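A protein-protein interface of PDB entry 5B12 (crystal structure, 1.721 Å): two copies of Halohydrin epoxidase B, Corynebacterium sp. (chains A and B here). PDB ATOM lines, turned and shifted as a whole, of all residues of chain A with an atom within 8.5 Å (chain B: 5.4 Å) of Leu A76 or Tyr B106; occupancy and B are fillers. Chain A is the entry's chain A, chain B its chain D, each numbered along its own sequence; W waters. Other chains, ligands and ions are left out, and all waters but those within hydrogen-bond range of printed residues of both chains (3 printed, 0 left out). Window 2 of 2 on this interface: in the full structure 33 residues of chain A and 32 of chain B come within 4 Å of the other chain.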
ATOM      1  N   GLY A  72      20.820  32.283 -25.481  1.00  0.00           N
ATOM      2  CA  GLY A  72      20.213  31.165 -24.800  1.00  0.00           C
ATOM      3  C   GLY A  72      18.901  31.497 -24.128  1.00  0.00           C
ATOM      4  O   GLY A  72      18.155  30.577 -23.779  1.00  0.00           O
ATOM      5  N   VAL A  73      18.602  32.787 -23.958  1.00  0.00           N
ATOM      6  CA  VAL A  73      17.337  33.196 -23.360  1.00  0.00           C
ATOM      7  C   VAL A  73      16.213  32.834 -24.322  1.00  0.00           C
ATOM      8  O   VAL A  73      16.306  33.086 -25.529  1.00  0.00           O
ATOM      9  CB  VAL A  73      17.359  34.696 -23.040  1.00  0.00           C
ATOM     10  CG1 VAL A  73      15.968  35.175 -22.620  1.00  0.00           C
ATOM     11  CG2 VAL A  73      18.367  34.998 -21.916  1.00  0.00           C
ATOM     12  N   THR A  74      15.172  32.184 -23.804  1.00  0.00           N
ATOM     13  CA  THR A  74      14.087  31.684 -24.639  1.00  0.00           C
ATOM     14  C   THR A  74      13.024  32.756 -24.884  1.00  0.00           C
ATOM     15  O   THR A  74      13.006  33.821 -24.258  1.00  0.00           O
ATOM     16  CB  THR A  74      13.389  30.501 -23.987  1.00  0.00           C
ATOM     17  OG1 THR A  74      12.712  30.992 -22.827  1.00  0.00           O
ATOM     18  CG2 THR A  74      14.360  29.398 -23.590  1.00  0.00           C
ATOM     19  N   VAL A  75      12.100  32.428 -25.793  1.00  0.00           N
ATOM     20  CA  VAL A  75      10.992  33.331 -26.092  1.00  0.00           C
ATOM     21  C   VAL A  75      10.192  33.616 -24.827  1.00  0.00           C
ATOM     22  O   VAL A  75       9.801  34.758 -24.575  1.00  0.00           O
ATOM     23  CB  VAL A  75      10.103  32.755 -27.210  1.00  0.00           C
ATOM     24  CG1 VAL A  75       9.501  31.395 -26.812  1.00  0.00           C
ATOM     25  CG2 VAL A  75       8.973  33.738 -27.540  1.00  0.00           C
ATOM     26  N   LEU A  76       9.958  32.594 -24.002  1.00  0.00           N
ATOM     27  CA  LEU A  76       9.153  32.824 -22.808  1.00  0.00           C
ATOM     28  C   LEU A  76       9.921  33.587 -21.757  1.00  0.00           C
ATOM     29  O   LEU A  76       9.303  34.253 -20.924  1.00  0.00           O
ATOM     30  CB  LEU A  76       8.624  31.501 -22.237  1.00  0.00           C
ATOM     31  CG  LEU A  76       7.760  30.704 -23.197  1.00  0.00           C
ATOM     32  CD1 LEU A  76       7.270  29.398 -22.525  1.00  0.00           C
ATOM     33  CD2 LEU A  76       6.583  31.576 -23.655  1.00  0.00           C
ATOM     34  N   GLU A  77      11.256  33.552 -21.809  1.00  0.00           N
ATOM     35  CA  GLU A  77      12.071  34.347 -20.901  1.00  0.00           C
ATOM     36  C   GLU A  77      12.344  35.744 -21.418  1.00  0.00           C
ATOM     37  O   GLU A  77      13.005  36.524 -20.721  1.00  0.00           O
ATOM     38  CB  GLU A  77      13.396  33.636 -20.640  1.00  0.00           C
ATOM     39  CG  GLU A  77      13.205  32.277 -19.991  1.00  0.00           C
ATOM     40  CD  GLU A  77      14.473  31.458 -20.032  1.00  0.00           C
ATOM     41  OE1 GLU A  77      15.400  31.859 -20.776  1.00  0.00           O
ATOM     42  OE2 GLU A  77      14.535  30.413 -19.340  1.00  0.00           O
ATOM     43  N   THR A  78      11.902  36.060 -22.640  1.00  0.00           N
ATOM     44  CA  THR A  78      12.168  37.370 -23.230  1.00  0.00           C
ATOM     45  C   THR A  78      11.103  38.323 -22.701  1.00  0.00           C
ATOM     46  O   THR A  78      10.028  38.473 -23.280  1.00  0.00           O
ATOM     47  CB  THR A  78      12.162  37.281 -24.755  1.00  0.00           C
ATOM     48  OG1 THR A  78      13.252  36.432 -25.159  1.00  0.00           O
ATOM     49  CG2 THR A  78      12.333  38.667 -25.361  1.00  0.00           C
ATOM     50  N   ASP A  79      11.386  38.929 -21.549  1.00  0.00           N
ATOM     51  CA  ASP A  79      10.386  39.763 -20.910  1.00  0.00           C
ATOM     52  C   ASP A  79      10.341  41.134 -21.577  1.00  0.00           C
ATOM     53  O   ASP A  79      11.121  41.441 -22.482  1.00  0.00           O
ATOM     54  CB  ASP A  79      10.626  39.847 -19.389  1.00  0.00           C
ATOM     55  CG  ASP A  79      11.960  40.505 -18.985  1.00  0.00           C
ATOM     56  OD1 ASP A  79      12.623  41.198 -19.777  1.00  0.00           O
ATOM     57  OD2 ASP A  79      12.330  40.350 -17.795  1.00  0.00           O
ATOM     58  N   GLU A  80       9.364  41.945 -21.147  1.00  0.00           N
ATOM     59  CA  GLU A  80       9.121  43.234 -21.767  1.00  0.00           C
ATOM     60  C   GLU A  80      10.383  44.092 -21.766  1.00  0.00           C
ATOM     61  O   GLU A  80      10.703  44.757 -22.759  1.00  0.00           O
ATOM     62  CB  GLU A  80       7.967  43.939 -21.030  1.00  0.00           C
ATOM     63  CG  GLU A  80       7.693  45.346 -21.528  1.00  0.00           C
ATOM     64  CD  GLU A  80       6.824  45.375 -22.771  1.00  0.00           C
ATOM     65  OE1 GLU A  80       6.090  44.398 -23.025  1.00  0.00           O
ATOM     66  OE2 GLU A  80       6.863  46.404 -23.474  1.00  0.00           O
ATOM     67  N   LEU A 129      16.349  35.695 -29.547  1.00  0.00           N
ATOM     68  CA  LEU A 129      15.097  36.102 -30.185  1.00  0.00           C
ATOM     69  C   LEU A 129      14.983  37.618 -30.320  1.00  0.00           C
ATOM     70  O   LEU A 129      14.843  38.141 -31.430  1.00  0.00           O
ATOM     71  CB  LEU A 129      13.902  35.542 -29.404  1.00  0.00           C
ATOM     72  CG  LEU A 129      12.567  36.137 -29.873  1.00  0.00           C
ATOM     73  CD1 LEU A 129      12.160  35.445 -31.151  1.00  0.00           C
ATOM     74  CD2 LEU A 129      11.505  35.961 -28.797  1.00  0.00           C
ATOM     75  N   ARG B  99       4.067  35.306 -26.986  1.00  0.00           N
ATOM     76  CA  ARG B  99       4.584  34.819 -25.711  1.00  0.00           C
ATOM     77  C   ARG B  99       3.446  34.356 -24.820  1.00  0.00           C
ATOM     78  O   ARG B  99       3.590  33.374 -24.086  1.00  0.00           O
ATOM     79  CB  ARG B  99       5.418  35.907 -25.034  1.00  0.00           C
ATOM     80  CG  ARG B  99       6.233  35.426 -23.786  1.00  0.00           C
ATOM     81  CD  ARG B  99       6.941  36.588 -23.083  1.00  0.00           C
ATOM     82  NE  ARG B  99       5.943  37.600 -22.706  1.00  0.00           N
ATOM     83  CZ  ARG B  99       6.118  38.909 -22.729  1.00  0.00           C
ATOM     84  NH1 ARG B  99       7.293  39.452 -23.069  1.00  0.00           N
ATOM     85  NH2 ARG B  99       5.091  39.702 -22.419  1.00  0.00           N
ATOM     86  N   LEU B 102       2.075  30.739 -26.364  1.00  0.00           N
ATOM     87  CA  LEU B 102       2.974  29.596 -26.432  1.00  0.00           C
ATOM     88  C   LEU B 102       2.914  28.650 -25.237  1.00  0.00           C
ATOM     89  O   LEU B 102       3.062  27.440 -25.458  1.00  0.00           O
ATOM     90  CB  LEU B 102       4.408  30.090 -26.627  1.00  0.00           C
ATOM     91  CG  LEU B 102       4.644  30.585 -28.060  1.00  0.00           C
ATOM     92  CD1 LEU B 102       5.987  31.348 -28.127  1.00  0.00           C
ATOM     93  CD2 LEU B 102       4.623  29.442 -29.034  1.00  0.00           C
ATOM     94  N   PRO B 103       2.760  29.096 -23.981  1.00  0.00           N
ATOM     95  CA  PRO B 103       2.780  28.103 -22.883  1.00  0.00           C
ATOM     96  C   PRO B 103       1.795  26.964 -23.082  1.00  0.00           C
ATOM     97  O   PRO B 103       2.148  25.787 -22.929  1.00  0.00           O
ATOM     98  CB  PRO B 103       2.463  28.946 -21.644  1.00  0.00           C
ATOM     99  CG  PRO B 103       2.991  30.321 -21.969  1.00  0.00           C
ATOM    100  CD  PRO B 103       2.661  30.472 -23.464  1.00  0.00           C
ATOM    101  N   GLN B 104       0.559  27.261 -23.468  1.00  0.00           N
ATOM    102  CA  GLN B 104      -0.365  26.151 -23.633  1.00  0.00           C
ATOM    103  C   GLN B 104      -0.007  25.284 -24.833  1.00  0.00           C
ATOM    104  O   GLN B 104      -0.175  24.065 -24.785  1.00  0.00           O
ATOM    105  CB  GLN B 104      -1.804  26.672 -23.702  1.00  0.00           C
ATOM    106  CG  GLN B 104      -2.191  27.417 -24.951  1.00  0.00           C
ATOM    107  CD  GLN B 104      -3.641  27.867 -24.857  1.00  0.00           C
ATOM    108  OE1 GLN B 104      -4.544  27.118 -25.199  1.00  0.00           O
ATOM    109  NE2 GLN B 104      -3.852  29.069 -24.374  1.00  0.00           N
ATOM    110  N   PHE B 105       0.517  25.885 -25.909  1.00  0.00           N
ATOM    111  CA  PHE B 105       1.069  25.094 -27.009  1.00  0.00           C
ATOM    112  C   PHE B 105       2.187  24.176 -26.535  1.00  0.00           C
ATOM    113  O   PHE B 105       2.302  23.037 -27.002  1.00  0.00           O
ATOM    114  CB  PHE B 105       1.624  26.020 -28.100  1.00  0.00           C
ATOM    115  CG  PHE B 105       0.572  26.757 -28.905  1.00  0.00           C
ATOM    116  CD1 PHE B 105      -0.779  26.438 -28.806  1.00  0.00           C
ATOM    117  CD2 PHE B 105       0.964  27.752 -29.799  1.00  0.00           C
ATOM    118  CE1 PHE B 105      -1.710  27.107 -29.582  1.00  0.00           C
ATOM    119  CE2 PHE B 105       0.025  28.423 -30.571  1.00  0.00           C
ATOM    120  CZ  PHE B 105      -1.309  28.094 -30.455  1.00  0.00           C
ATOM    121  N   TYR B 106       3.047  24.668 -25.639  1.00  0.00           N
ATOM    122  CA  TYR B 106       4.176  23.860 -25.185  1.00  0.00           C
ATOM    123  C   TYR B 106       3.728  22.695 -24.305  1.00  0.00           C
ATOM    124  O   TYR B 106       4.334  21.621 -24.351  1.00  0.00           O
ATOM    125  CB  TYR B 106       5.184  24.738 -24.425  1.00  0.00           C
ATOM    126  CG  TYR B 106       6.013  25.628 -25.333  1.00  0.00           C
ATOM    127  CD1 TYR B 106       5.880  25.553 -26.709  1.00  0.00           C
ATOM    128  CD2 TYR B 106       6.946  26.512 -24.800  1.00  0.00           C
ATOM    129  CE1 TYR B 106       6.669  26.351 -27.552  1.00  0.00           C
ATOM    130  CE2 TYR B 106       7.728  27.317 -25.620  1.00  0.00           C
ATOM    131  CZ  TYR B 106       7.589  27.218 -26.986  1.00  0.00           C
ATOM    132  OH  TYR B 106       8.390  28.021 -27.782  1.00  0.00           O
ATOM    133  N   GLU B 107       2.683  22.884 -23.490  1.00  0.00           N
ATOM    134  CA  GLU B 107       2.151  21.743 -22.740  1.00  0.00           C
ATOM    135  C   GLU B 107       1.639  20.659 -23.676  1.00  0.00           C
ATOM    136  O   GLU B 107       1.904  19.466 -23.466  1.00  0.00           O
ATOM    137  CB  GLU B 107       1.036  22.166 -21.777  1.00  0.00           C
ATOM    138  CG  GLU B 107       0.530  20.946 -21.001  1.00  0.00           C
ATOM    139  CD  GLU B 107      -0.565  21.264 -19.985  1.00  0.00           C
ATOM    140  OE1 GLU B 107      -1.554  21.955 -20.338  1.00  0.00           O
ATOM    141  OE2 GLU B 107      -0.436  20.800 -18.822  1.00  0.00           O
ATOM    142  N   ARG B 108       0.901  21.051 -24.728  1.00  0.00           N
ATOM    143  CA  ARG B 108       0.324  20.060 -25.616  1.00  0.00           C
ATOM    144  C   ARG B 108       1.272  19.628 -26.720  1.00  0.00           C
ATOM    145  O   ARG B 108       0.960  18.676 -27.438  1.00  0.00           O
ATOM    146  CB  ARG B 108      -0.954  20.617 -26.264  1.00  0.00           C
ATOM    147  CG  ARG B 108      -2.026  20.958 -25.278  1.00  0.00           C
ATOM    148  CD  ARG B 108      -3.335  21.281 -25.993  1.00  0.00           C
ATOM    149  NE  ARG B 108      -3.335  22.580 -26.658  1.00  0.00           N
ATOM    150  CZ  ARG B 108      -3.655  23.731 -26.074  1.00  0.00           C
ATOM    151  NH1 ARG B 108      -3.979  23.778 -24.780  1.00  0.00           N
ATOM    152  NH2 ARG B 108      -3.656  24.842 -26.783  1.00  0.00           N
ATOM    153  N   ASN B 109       2.400  20.327 -26.876  1.00  0.00           N
ATOM    154  CA  ASN B 109       3.295  20.061 -27.994  1.00  0.00           C
ATOM    155  C   ASN B 109       2.540  20.152 -29.319  1.00  0.00           C
ATOM    156  O   ASN B 109       2.618  19.250 -30.154  1.00  0.00           O
ATOM    157  CB  ASN B 109       3.957  18.691 -27.844  1.00  0.00           C
ATOM    158  CG  ASN B 109       5.354  18.654 -28.420  1.00  0.00           C
ATOM    159  OD1 ASN B 109       6.271  19.240 -27.856  1.00  0.00           O
ATOM    160  ND2 ASN B 109       5.527  17.949 -29.531  1.00  0.00           N
ATOM    161  N   LYS B 110       1.786  21.236 -29.485  1.00  0.00           N
ATOM    162  CA  LYS B 110       1.026  21.505 -30.700  1.00  0.00           C
ATOM    163  C   LYS B 110       0.585  22.952 -30.678  1.00  0.00           C
ATOM    164  O   LYS B 110       0.091  23.442 -29.655  1.00  0.00           O
ATOM    165  CB  LYS B 110      -0.189  20.568 -30.819  1.00  0.00           C
ATOM    166  CG  LYS B 110      -1.031  20.826 -32.070  1.00  0.00           C
ATOM    167  CD  LYS B 110      -0.304  20.415 -33.327  1.00  0.00           C
ATOM    168  CE  LYS B 110      -1.033  20.909 -34.584  1.00  0.00           C
ATOM    169  NZ  LYS B 110      -0.431  20.352 -35.852  1.00  0.00           N
ATOM    170  N   LEU B 145      11.443  32.998 -34.038  1.00  0.00           N
ATOM    171  CA  LEU B 145      10.612  32.151 -33.187  1.00  0.00           C
ATOM    172  C   LEU B 145      10.302  30.824 -33.852  1.00  0.00           C
ATOM    173  O   LEU B 145      10.250  29.788 -33.184  1.00  0.00           O
ATOM    174  CB  LEU B 145       9.306  32.861 -32.824  1.00  0.00           C
ATOM    175  CG  LEU B 145       8.318  31.989 -32.038  1.00  0.00           C
ATOM    176  CD1 LEU B 145       8.971  31.487 -30.717  1.00  0.00           C
ATOM    177  CD2 LEU B 145       7.033  32.798 -31.765  1.00  0.00           C
ATOM    178  N   GLU B 148      12.493  27.867 -33.060  1.00  0.00           N
ATOM    179  CA  GLU B 148      12.472  27.620 -31.620  1.00  0.00           C
ATOM    180  C   GLU B 148      11.181  26.896 -31.232  1.00  0.00           C
ATOM    181  O   GLU B 148      11.207  25.835 -30.584  1.00  0.00           O
ATOM    182  CB  GLU B 148      12.604  28.953 -30.874  1.00  0.00           C
ATOM    183  CG  GLU B 148      12.442  28.796 -29.363  1.00  0.00           C
ATOM    184  CD  GLU B 148      12.673  30.079 -28.580  1.00  0.00           C
ATOM    185  OE1 GLU B 148      13.057  31.117 -29.174  1.00  0.00           O
ATOM    186  OE2 GLU B 148      12.497  30.043 -27.348  1.00  0.00           O
ATOM    187  N   ALA B 149      10.052  27.432 -31.696  1.00  0.00           N
ATOM    188  CA  ALA B 149       8.734  26.845 -31.426  1.00  0.00           C
ATOM    189  C   ALA B 149       8.533  25.497 -32.103  1.00  0.00           C
ATOM    190  O   ALA B 149       7.802  24.634 -31.587  1.00  0.00           O
ATOM    191  CB  ALA B 149       7.656  27.838 -31.881  1.00  0.00           C
ATOM    192  N   HIS B 152       8.719  22.287 -30.300  1.00  0.00           N
ATOM    193  CA  HIS B 152       7.499  21.898 -29.600  1.00  0.00           C
ATOM    194  C   HIS B 152       6.333  21.628 -30.544  1.00  0.00           C
ATOM    195  O   HIS B 152       5.179  21.694 -30.105  1.00  0.00           O
ATOM    196  CB  HIS B 152       7.096  22.975 -28.614  1.00  0.00           C
ATOM    197  CG  HIS B 152       8.119  23.235 -27.559  1.00  0.00           C
ATOM    198  ND1 HIS B 152       8.162  22.524 -26.376  1.00  0.00           N
ATOM    199  CD2 HIS B 152       9.150  24.112 -27.514  1.00  0.00           C
ATOM    200  CE1 HIS B 152       9.166  22.972 -25.638  1.00  0.00           C
ATOM    201  NE2 HIS B 152       9.780  23.934 -26.304  1.00  0.00           N
ATOM    202  N   VAL B 154       5.118  23.461 -32.861  1.00  0.00           N
ATOM    203  CA  VAL B 154       4.321  24.678 -33.023  1.00  0.00           C
ATOM    204  C   VAL B 154       4.769  25.340 -34.317  1.00  0.00           C
ATOM    205  O   VAL B 154       5.969  25.582 -34.499  1.00  0.00           O
ATOM    206  CB  VAL B 154       4.496  25.651 -31.855  1.00  0.00           C
ATOM    207  CG1 VAL B 154       3.851  26.971 -32.191  1.00  0.00           C
ATOM    208  CG2 VAL B 154       3.900  25.089 -30.552  1.00  0.00           C
HETATM  209  O   HOH W   1       4.668  42.339 -21.766  1.00  0.00           O
HETATM  210  O   HOH W   2      15.424  32.701 -28.175  1.00  0.00           O
HETATM  211  O   HOH W   3       7.069  42.000 -24.278  1.00  0.00           O
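No position is printed for both chains.
Of the 13 pairs that touch across the chains among the printed residues, none has its exchanged pair printed and touching as well.
N of Val A75 lies within hydrogen-bond range of OE2 of Glu B148, at 2.9 Å.
O of Thr A78 is in hydrogen-bond range of NH1 of Arg B99, 2.9 Å away.
The backbone NH (N) of Leu A76 sits close to the side-chain hydroxyl (OG1) of Thr A74 (3.4 Å).
The side-chain carboxylate (OE1) of Glu A77 sits at hydrogen-bond distance from the backbone NH (N) of Thr A74 (3.1 Å).
The side-chain hydroxyl (OG1) of Thr A78 is in hydrogen-bond range of the backbone carbonyl oxygen (O) of Thr A74, 2.8 Å away.
Among the printed residues, 13 pairs touch across the chains.
Among the printed residues, no Asp or Glu carboxylate lies within 4 Å of a Lys or Arg side-chain nitrogen of the other chain.
Thr A74 touches Glu B148 (CB to OE2, 3.5 Å).
Val A75 touches Leu B102.
Val A75 touches Tyr B106 (CG1 to OH, 3.7 Å).
CD1 of Leu B145 touches CG2 of Val A75, at 3.9 Å.
Leu A76 touches Arg B99.
CB of Leu B102 touches CD2 of Leu A76, at 3.97 Å.
Leu A76 touches Tyr B106.
Arg B99 touches Asp A79.
Arg B99 touches Glu A80.
Leu A129 touches Leu B145.
Water W1 lies within hydrogen-bond range of NH2 of Arg B99 (2.7 Å) and OE1 of Glu A80 (2.8 Å).
Water W2 lies within hydrogen-bond range of O of Val A73 (2.8 Å), OE1 of Glu B148 (3.0 Å) and N of Leu A129 (3.4 Å).
Water W3 lies within hydrogen-bond range of the guanidinium group (NH1) of Arg B99 (2.8 Å) and the side-chain carboxylate (OE1) of Glu A80 (2.9 Å).
Of chain B, only Arg B99, Leu B102 and Tyr B106 come within 4 Å of Leu A76.
Of the printed residues of chain B, Glu A80 touches Arg B99.
Of chain A, only Val A75 and Leu A76 come within 4 Å of Tyr B106.
Of the printed residues of chain A, Leu B145 touches Val A75 and Leu A129.
His B152 touches none of the printed residues of chain A.
The nearest residue of chain A that does not touch Tyr B106 is Thr A74 (6.7 Å).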
